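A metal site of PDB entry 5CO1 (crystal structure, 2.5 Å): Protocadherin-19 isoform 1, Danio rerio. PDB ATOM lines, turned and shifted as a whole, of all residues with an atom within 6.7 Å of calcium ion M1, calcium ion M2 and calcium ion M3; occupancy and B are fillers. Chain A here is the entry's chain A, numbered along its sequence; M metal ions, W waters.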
ATOM      1  N   GLU A  15      11.138 -26.472   9.374  1.00  0.00           N
ATOM      2  CA  GLU A  15      11.961 -27.542   9.904  1.00  0.00           C
ATOM      3  C   GLU A  15      12.814 -26.973  11.009  1.00  0.00           C
ATOM      4  O   GLU A  15      13.043 -25.775  11.056  1.00  0.00           O
ATOM      5  CB  GLU A  15      12.802 -28.242   8.852  1.00  0.00           C
ATOM      6  CG  GLU A  15      13.979 -27.478   8.305  1.00  0.00           C
ATOM      7  CD  GLU A  15      14.787 -28.323   7.348  1.00  0.00           C
ATOM      8  OE1 GLU A  15      15.062 -29.504   7.695  1.00  0.00           O
ATOM      9  OE2 GLU A  15      15.093 -27.843   6.225  1.00  0.00           O
ATOM     10  N   ASN A  16      13.066 -27.850  11.986  1.00  0.00           N
ATOM     11  CA  ASN A  16      13.921 -27.577  13.134  1.00  0.00           C
ATOM     12  C   ASN A  16      13.230 -26.672  14.130  1.00  0.00           C
ATOM     13  O   ASN A  16      13.841 -26.113  15.031  1.00  0.00           O
ATOM     14  CB  ASN A  16      15.272 -27.013  12.704  1.00  0.00           C
ATOM     15  CG  ASN A  16      16.048 -27.964  11.781  1.00  0.00           C
ATOM     16  OD1 ASN A  16      15.901 -29.196  11.835  1.00  0.00           O
ATOM     17  ND2 ASN A  16      16.876 -27.387  10.911  1.00  0.00           N
ATOM     18  N   LEU A  70      11.912 -31.996  13.706  1.00  0.00           N
ATOM     19  CA  LEU A  70      11.334 -31.987  12.368  1.00  0.00           C
ATOM     20  C   LEU A  70      12.386 -31.733  11.323  1.00  0.00           C
ATOM     21  O   LEU A  70      12.908 -30.611  11.243  1.00  0.00           O
ATOM     22  CB  LEU A  70      10.316 -30.879  12.247  1.00  0.00           C
ATOM     23  CG  LEU A  70       8.982 -31.073  12.938  1.00  0.00           C
ATOM     24  CD1 LEU A  70       8.143 -29.852  12.673  1.00  0.00           C
ATOM     25  CD2 LEU A  70       8.272 -32.315  12.434  1.00  0.00           C
ATOM     26  N   ASP A  71      12.622 -32.710  10.450  1.00  0.00           N
ATOM     27  CA  ASP A  71      13.682 -32.623   9.445  1.00  0.00           C
ATOM     28  C   ASP A  71      13.074 -32.817   8.086  1.00  0.00           C
ATOM     29  O   ASP A  71      12.538 -33.887   7.803  1.00  0.00           O
ATOM     30  CB  ASP A  71      14.744 -33.671   9.720  1.00  0.00           C
ATOM     31  CG  ASP A  71      15.915 -33.617   8.719  1.00  0.00           C
ATOM     32  OD1 ASP A  71      15.993 -32.709   7.875  1.00  0.00           O
ATOM     33  OD2 ASP A  71      16.749 -34.541   8.787  1.00  0.00           O
ATOM     34  N   HIS A  72      13.075 -31.740   7.286  1.00  0.00           N
ATOM     35  CA  HIS A  72      12.592 -31.798   5.910  1.00  0.00           C
ATOM     36  C   HIS A  72      13.287 -32.889   5.087  1.00  0.00           C
ATOM     37  O   HIS A  72      12.698 -33.468   4.166  1.00  0.00           O
ATOM     38  CB  HIS A  72      12.812 -30.459   5.218  1.00  0.00           C
ATOM     39  CG  HIS A  72      12.474 -30.467   3.764  1.00  0.00           C
ATOM     40  ND1 HIS A  72      11.226 -30.142   3.298  1.00  0.00           N
ATOM     41  CD2 HIS A  72      13.226 -30.745   2.674  1.00  0.00           C
ATOM     42  CE1 HIS A  72      11.223 -30.185   1.972  1.00  0.00           C
ATOM     43  NE2 HIS A  72      12.426 -30.547   1.572  1.00  0.00           N
ATOM     44  N   GLU A  73      14.573 -33.084   5.342  1.00  0.00           N
ATOM     45  CA  GLU A  73      15.359 -34.019   4.516  1.00  0.00           C
ATOM     46  C   GLU A  73      14.986 -35.490   4.868  1.00  0.00           C
ATOM     47  O   GLU A  73      15.054 -36.374   4.012  1.00  0.00           O
ATOM     48  CB  GLU A  73      16.857 -33.736   4.657  1.00  0.00           C
ATOM     49  CG  GLU A  73      17.303 -32.461   3.941  1.00  0.00           C
ATOM     50  CD  GLU A  73      16.851 -31.149   4.619  1.00  0.00           C
ATOM     51  OE1 GLU A  73      16.962 -31.015   5.867  1.00  0.00           O
ATOM     52  OE2 GLU A  73      16.406 -30.221   3.887  1.00  0.00           O
ATOM     53  N   GLU A  74      14.451 -35.684   6.074  1.00  0.00           N
ATOM     54  CA  GLU A  74      13.880 -36.952   6.516  1.00  0.00           C
ATOM     55  C   GLU A  74      12.441 -37.179   6.037  1.00  0.00           C
ATOM     56  O   GLU A  74      12.085 -38.290   5.708  1.00  0.00           O
ATOM     57  CB  GLU A  74      13.952 -36.989   8.036  1.00  0.00           C
ATOM     58  CG  GLU A  74      13.541 -38.293   8.695  1.00  0.00           C
ATOM     59  CD  GLU A  74      13.422 -38.164  10.219  1.00  0.00           C
ATOM     60  OE1 GLU A  74      13.212 -39.182  10.898  1.00  0.00           O
ATOM     61  OE2 GLU A  74      13.529 -37.021  10.734  1.00  0.00           O
ATOM     62  N   ILE A 103       8.663 -27.142   6.211  1.00  0.00           N
ATOM     63  CA  ILE A 103       9.218 -26.243   5.237  1.00  0.00           C
ATOM     64  C   ILE A 103      10.731 -26.221   5.310  1.00  0.00           C
ATOM     65  O   ILE A 103      11.312 -26.215   6.374  1.00  0.00           O
ATOM     66  CB  ILE A 103       8.501 -24.888   5.312  1.00  0.00           C
ATOM     67  CG1 ILE A 103       7.156 -25.109   4.638  1.00  0.00           C
ATOM     68  CG2 ILE A 103       9.236 -23.812   4.504  1.00  0.00           C
ATOM     69  CD1 ILE A 103       6.082 -24.279   5.231  1.00  0.00           C
ATOM     70  N   ASP A 104      11.337 -26.400   4.157  1.00  0.00           N
ATOM     71  CA  ASP A 104      12.776 -26.599   4.077  1.00  0.00           C
ATOM     72  C   ASP A 104      13.490 -25.282   4.316  1.00  0.00           C
ATOM     73  O   ASP A 104      13.050 -24.224   3.829  1.00  0.00           O
ATOM     74  CB  ASP A 104      13.155 -27.167   2.721  1.00  0.00           C
ATOM     75  CG  ASP A 104      14.636 -27.060   2.438  1.00  0.00           C
ATOM     76  OD1 ASP A 104      15.425 -27.681   3.194  1.00  0.00           O
ATOM     77  OD2 ASP A 104      15.002 -26.399   1.438  1.00  0.00           O
ATOM     78  N   ILE A 105      14.483 -25.340   5.196  1.00  0.00           N
ATOM     79  CA  ILE A 105      15.519 -24.327   5.303  1.00  0.00           C
ATOM     80  C   ILE A 105      16.910 -24.812   4.933  1.00  0.00           C
ATOM     81  O   ILE A 105      17.165 -26.019   4.801  1.00  0.00           O
ATOM     82  CB  ILE A 105      15.577 -23.745   6.726  1.00  0.00           C
ATOM     83  CG1 ILE A 105      15.851 -24.849   7.740  1.00  0.00           C
ATOM     84  CG2 ILE A 105      14.273 -23.017   7.053  1.00  0.00           C
ATOM     85  CD1 ILE A 105      16.928 -24.506   8.724  1.00  0.00           C
ATOM     86  N   ASN A 106      17.806 -23.853   4.698  1.00  0.00           N
ATOM     87  CA  ASN A 106      19.164 -24.170   4.355  1.00  0.00           C
ATOM     88  C   ASN A 106      19.997 -24.606   5.564  1.00  0.00           C
ATOM     89  O   ASN A 106      20.799 -23.872   6.071  1.00  0.00           O
ATOM     90  CB  ASN A 106      19.818 -23.002   3.694  1.00  0.00           C
ATOM     91  CG  ASN A 106      20.937 -23.432   2.780  1.00  0.00           C
ATOM     92  OD1 ASN A 106      21.050 -24.593   2.424  1.00  0.00           O
ATOM     93  ND2 ASN A 106      21.748 -22.482   2.364  1.00  0.00           N
ATOM     94  N   ASP A 107      19.827 -25.834   5.989  1.00  0.00           N
ATOM     95  CA  ASP A 107      20.640 -26.387   7.054  1.00  0.00           C
ATOM     96  C   ASP A 107      21.643 -27.436   6.527  1.00  0.00           C
ATOM     97  O   ASP A 107      22.095 -28.268   7.273  1.00  0.00           O
ATOM     98  CB  ASP A 107      19.732 -26.989   8.139  1.00  0.00           C
ATOM     99  CG  ASP A 107      18.772 -28.056   7.616  1.00  0.00           C
ATOM    100  OD1 ASP A 107      18.450 -28.052   6.403  1.00  0.00           O
ATOM    101  OD2 ASP A 107      18.257 -28.851   8.430  1.00  0.00           O
ATOM    102  N   ASN A 108      21.955 -27.414   5.234  1.00  0.00           N
ATOM    103  CA  ASN A 108      22.886 -28.387   4.643  1.00  0.00           C
ATOM    104  C   ASN A 108      23.816 -27.713   3.690  1.00  0.00           C
ATOM    105  O   ASN A 108      23.385 -27.145   2.695  1.00  0.00           O
ATOM    106  CB  ASN A 108      22.148 -29.492   3.882  1.00  0.00           C
ATOM    107  CG  ASN A 108      21.594 -30.577   4.789  1.00  0.00           C
ATOM    108  OD1 ASN A 108      22.350 -31.400   5.284  1.00  0.00           O
ATOM    109  ND2 ASN A 108      20.292 -30.510   5.098  1.00  0.00           N
ATOM    110  N   ALA A 109      25.100 -27.822   3.980  1.00  0.00           N
ATOM    111  CA  ALA A 109      26.170 -27.294   3.143  1.00  0.00           C
ATOM    112  C   ALA A 109      26.354 -28.183   1.928  1.00  0.00           C
ATOM    113  O   ALA A 109      25.938 -29.345   1.925  1.00  0.00           O
ATOM    114  CB  ALA A 109      27.461 -27.246   3.943  1.00  0.00           C
ATOM    115  N   PRO A 110      27.009 -27.654   0.887  1.00  0.00           N
ATOM    116  CA  PRO A 110      27.256 -28.485  -0.286  1.00  0.00           C
ATOM    117  C   PRO A 110      28.318 -29.530  -0.033  1.00  0.00           C
ATOM    118  O   PRO A 110      29.286 -29.222   0.650  1.00  0.00           O
ATOM    119  CB  PRO A 110      27.726 -27.491  -1.344  1.00  0.00           C
ATOM    120  CG  PRO A 110      27.195 -26.179  -0.921  1.00  0.00           C
ATOM    121  CD  PRO A 110      27.109 -26.218   0.575  1.00  0.00           C
ATOM    122  N   ASP A 141      23.736 -31.118  -2.656  1.00  0.00           N
ATOM    123  CA  ASP A 141      23.197 -30.488  -1.490  1.00  0.00           C
ATOM    124  C   ASP A 141      21.885 -31.208  -1.186  1.00  0.00           C
ATOM    125  O   ASP A 141      20.984 -31.261  -2.019  1.00  0.00           O
ATOM    126  CB  ASP A 141      22.941 -28.990  -1.792  1.00  0.00           C
ATOM    127  CG  ASP A 141      22.868 -28.112  -0.534  1.00  0.00           C
ATOM    128  OD1 ASP A 141      21.977 -28.342   0.302  1.00  0.00           O
ATOM    129  OD2 ASP A 141      23.639 -27.136  -0.428  1.00  0.00           O
ATOM    130  N   ASN A 142      21.772 -31.722   0.025  1.00  0.00           N
ATOM    131  CA  ASN A 142      20.547 -32.354   0.472  1.00  0.00           C
ATOM    132  C   ASN A 142      19.318 -31.451   0.614  1.00  0.00           C
ATOM    133  O   ASN A 142      18.251 -31.957   0.894  1.00  0.00           O
ATOM    134  CB  ASN A 142      20.761 -33.075   1.814  1.00  0.00           C
ATOM    135  CG  ASN A 142      21.923 -34.055   1.763  1.00  0.00           C
ATOM    136  OD1 ASN A 142      22.031 -34.853   0.849  1.00  0.00           O
ATOM    137  ND2 ASN A 142      22.826 -33.937   2.724  1.00  0.00           N
ATOM    138  N   ASP A 143      19.476 -30.123   0.542  1.00  0.00           N
ATOM    139  CA  ASP A 143      18.318 -29.211   0.696  1.00  0.00           C
ATOM    140  C   ASP A 143      17.558 -29.151  -0.632  1.00  0.00           C
ATOM    141  O   ASP A 143      18.065 -29.621  -1.649  1.00  0.00           O
ATOM    142  CB  ASP A 143      18.751 -27.784   1.136  1.00  0.00           C
ATOM    143  CG  ASP A 143      19.470 -27.756   2.484  1.00  0.00           C
ATOM    144  OD1 ASP A 143      18.908 -28.304   3.476  1.00  0.00           O
ATOM    145  OD2 ASP A 143      20.586 -27.171   2.551  1.00  0.00           O
ATOM    146  N   SER A 144      16.376 -28.531  -0.628  1.00  0.00           N
ATOM    147  CA  SER A 144      15.591 -28.342  -1.853  1.00  0.00           C
ATOM    148  C   SER A 144      15.577 -26.908  -2.367  1.00  0.00           C
ATOM    149  O   SER A 144      16.133 -26.008  -1.768  1.00  0.00           O
ATOM    150  CB  SER A 144      14.153 -28.806  -1.606  1.00  0.00           C
ATOM    151  OG  SER A 144      14.167 -30.103  -1.013  1.00  0.00           O
ATOM    152  N   ALA A 146      16.378 -23.458  -4.149  1.00  0.00           N
ATOM    153  CA  ALA A 146      17.584 -22.643  -4.154  1.00  0.00           C
ATOM    154  C   ALA A 146      18.570 -23.116  -3.099  1.00  0.00           C
ATOM    155  O   ALA A 146      19.778 -23.008  -3.296  1.00  0.00           O
ATOM    156  CB  ALA A 146      17.218 -21.188  -3.878  1.00  0.00           C
ATOM    157  N   ASN A 147      18.044 -23.578  -1.972  1.00  0.00           N
ATOM    158  CA  ASN A 147      18.900 -24.006  -0.865  1.00  0.00           C
ATOM    159  C   ASN A 147      19.785 -25.139  -1.286  1.00  0.00           C
ATOM    160  O   ASN A 147      20.758 -25.457  -0.584  1.00  0.00           O
ATOM    161  CB  ASN A 147      18.069 -24.506   0.270  1.00  0.00           C
ATOM    162  CG  ASN A 147      17.286 -23.412   0.942  1.00  0.00           C
ATOM    163  OD1 ASN A 147      17.742 -22.280   1.042  1.00  0.00           O
ATOM    164  ND2 ASN A 147      16.206 -23.809   1.617  1.00  0.00           N
ATOM    165  N   GLY A 148      19.308 -25.874  -2.283  1.00  0.00           N
ATOM    166  CA  GLY A 148      20.019 -27.018  -2.829  1.00  0.00           C
ATOM    167  C   GLY A 148      20.756 -26.845  -4.154  1.00  0.00           C
ATOM    168  O   GLY A 148      21.483 -27.750  -4.530  1.00  0.00           O
ATOM    169  N   LYS A 149      20.510 -25.745  -4.896  1.00  0.00           N
ATOM    170  CA  LYS A 149      21.279 -25.374  -6.100  1.00  0.00           C
ATOM    171  C   LYS A 149      22.675 -24.882  -5.739  1.00  0.00           C
ATOM    172  O   LYS A 149      22.814 -23.835  -5.137  1.00  0.00           O
ATOM    173  CB  LYS A 149      20.615 -24.238  -6.892  1.00  0.00           C
ATOM    174  CG  LYS A 149      19.362 -24.632  -7.669  1.00  0.00           C
ATOM    175  CD  LYS A 149      19.615 -24.730  -9.184  1.00  0.00           C
ATOM    176  CE  LYS A 149      18.780 -25.840  -9.827  1.00  0.00           C
ATOM    177  NZ  LYS A 149      17.372 -25.905  -9.309  1.00  0.00           N
ATOM    178  N   VAL A 150      23.675 -25.491  -6.353  1.00  0.00           N
ATOM    179  CA  VAL A 150      25.054 -25.317  -5.960  1.00  0.00           C
ATOM    180  C   VAL A 150      25.884 -24.838  -7.134  1.00  0.00           C
ATOM    181  O   VAL A 150      25.494 -24.984  -8.262  1.00  0.00           O
ATOM    182  CB  VAL A 150      25.621 -26.662  -5.505  1.00  0.00           C
ATOM    183  CG1 VAL A 150      27.127 -26.593  -5.304  1.00  0.00           C
ATOM    184  CG2 VAL A 150      24.922 -27.063  -4.225  1.00  0.00           C
ATOM    185  N   ASP A 193      26.019 -22.769  -2.233  1.00  0.00           N
ATOM    186  CA  ASP A 193      24.633 -22.965  -2.547  1.00  0.00           C
ATOM    187  C   ASP A 193      23.955 -21.634  -2.584  1.00  0.00           C
ATOM    188  O   ASP A 193      24.607 -20.630  -2.396  1.00  0.00           O
ATOM    189  CB  ASP A 193      23.982 -23.913  -1.543  1.00  0.00           C
ATOM    190  CG  ASP A 193      23.720 -23.261  -0.207  1.00  0.00           C
ATOM    191  OD1 ASP A 193      23.466 -22.032  -0.198  1.00  0.00           O
ATOM    192  OD2 ASP A 193      23.692 -24.014   0.806  1.00  0.00           O
ATOM    193  N   SER A 194      22.686 -21.589  -2.941  1.00  0.00           N
ATOM    194  CA  SER A 194      22.040 -20.330  -3.276  1.00  0.00           C
ATOM    195  C   SER A 194      20.900 -20.034  -2.319  1.00  0.00           C
ATOM    196  O   SER A 194      19.983 -19.275  -2.630  1.00  0.00           O
ATOM    197  CB  SER A 194      21.531 -20.395  -4.704  1.00  0.00           C
ATOM    198  OG  SER A 194      22.567 -20.886  -5.525  1.00  0.00           O
ATOM    199  N   GLY A 195      20.933 -20.698  -1.174  1.00  0.00           N
ATOM    200  CA  GLY A 195      20.030 -20.418  -0.084  1.00  0.00           C
ATOM    201  C   GLY A 195      20.427 -19.153   0.639  1.00  0.00           C
ATOM    202  O   GLY A 195      21.359 -18.460   0.236  1.00  0.00           O
ATOM    203  N   LEU A 199      25.400 -21.202   2.322  1.00  0.00           N
ATOM    204  CA  LEU A 199      26.366 -22.033   2.982  1.00  0.00           C
ATOM    205  C   LEU A 199      27.401 -22.487   1.967  1.00  0.00           C
ATOM    206  O   LEU A 199      27.129 -22.602   0.766  1.00  0.00           O
ATOM    207  CB  LEU A 199      25.693 -23.271   3.565  1.00  0.00           C
ATOM    208  CG  LEU A 199      24.771 -23.113   4.772  1.00  0.00           C
ATOM    209  CD1 LEU A 199      24.042 -24.426   5.026  1.00  0.00           C
ATOM    210  CD2 LEU A 199      25.533 -22.691   6.006  1.00  0.00           C
HETATM  211 CA    CA M   1      22.156 -26.101   1.134  1.00  0.00          CA
HETATM  212 CA    CA M   2      16.863 -28.220   4.838  1.00  0.00          CA
HETATM  213 CA    CA M   3      17.209 -30.654   7.938  1.00  0.00          CA
HETATM  214  O   HOH W   1      16.920 -31.236  10.110  1.00  0.00           O
HETATM  215  O   HOH W   2      19.263 -31.864   7.672  1.00  0.00           O
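Calcium ion M3 is bound by OE1 of Glu 73 (2.1 Å), OD2 of Asp 107 (2.1 Å), water W1 (2.3 Å), OD1 of Asp 71 (2.4 Å), water W2 (2.4 Å) and OE1 of Glu 15 (2.4 Å).
Calcium ion M3 has six donor atoms within binding distance.
Along chain A the residues within 4 Å of calcium ion M2 span positions 15 to 143.
Four residues have an atom within 4 Å of calcium ion M3: Glu 15, Asp 71, Glu 73 and Asp 107.
The nearest printed residue that does not touch calcium ion M3 is Asn 108 (4.2 Å).
N of Asp 193 sits at hydrogen-bond distance from O of Leu 199, at 3.2 Å.
The backbone carbonyl oxygen (O) of Ile 103 is in hydrogen-bond range of the backbone NH (N) of Glu 15 (3.0 Å).
The backbone NH (N) of Gly 195 lies within hydrogen-bond range of the side-chain carboxylate (OD1) of Asp 193.
OD2 of Asp 104 sits at hydrogen-bond distance from N of Ser 144, at 3.3 Å.
ND2 of Asn 108 lies close to OD1 of Asp 107 (3.3 Å).
The side-chain amide nitrogen (ND2) of Asn 147 is in hydrogen-bond range of the side-chain carboxylate (OD2) of Asp 104 (2.9 Å).
OE1 of Glu 15 sits close to N of His 72, 3.0 Å away.
OE1 of Glu 73 lies close to ND2 of Asn 108, 3.5 Å away.
Six residues have an atom within 4 Å of calcium ion M1: Asn 106, Asn 108, Asp 141, Asp 143, Asn 147 and Asp 193.
The nearest printed residue that does not touch calcium ion M1 is Ala 109 (4.4 Å).
Calcium ion M2 is bound by O of Ile 105 (2.2 Å), OD1 of Asp 107 (2.2 Å), OD1 of Asp 104 (2.2 Å), OE2 of Glu 73 (2.3 Å), OE2 of Glu 15 (2.3 Å) and OD1 of Asp 143 (2.5 Å).
Slightly farther from calcium ion M2 lies the side-chain carboxylate (OE1) of Glu 73 (3.0 Å).
Calcium ion M1 is bound by the backbone carbonyl oxygen (O) of Asn 108, the side-chain amide oxygen (OD1) of Asn 106, the backbone carbonyl oxygen (O) of Asn 147, the side-chain carboxylate (OD2) of Asp 143, the side-chain carboxylate (OD2) of Asp 141, the side-chain carboxylate (OD1) of Asp 141 and the side-chain carboxylate (OD2) of Asp 193.
Calcium ion M1 has seven donor atoms within binding distance.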
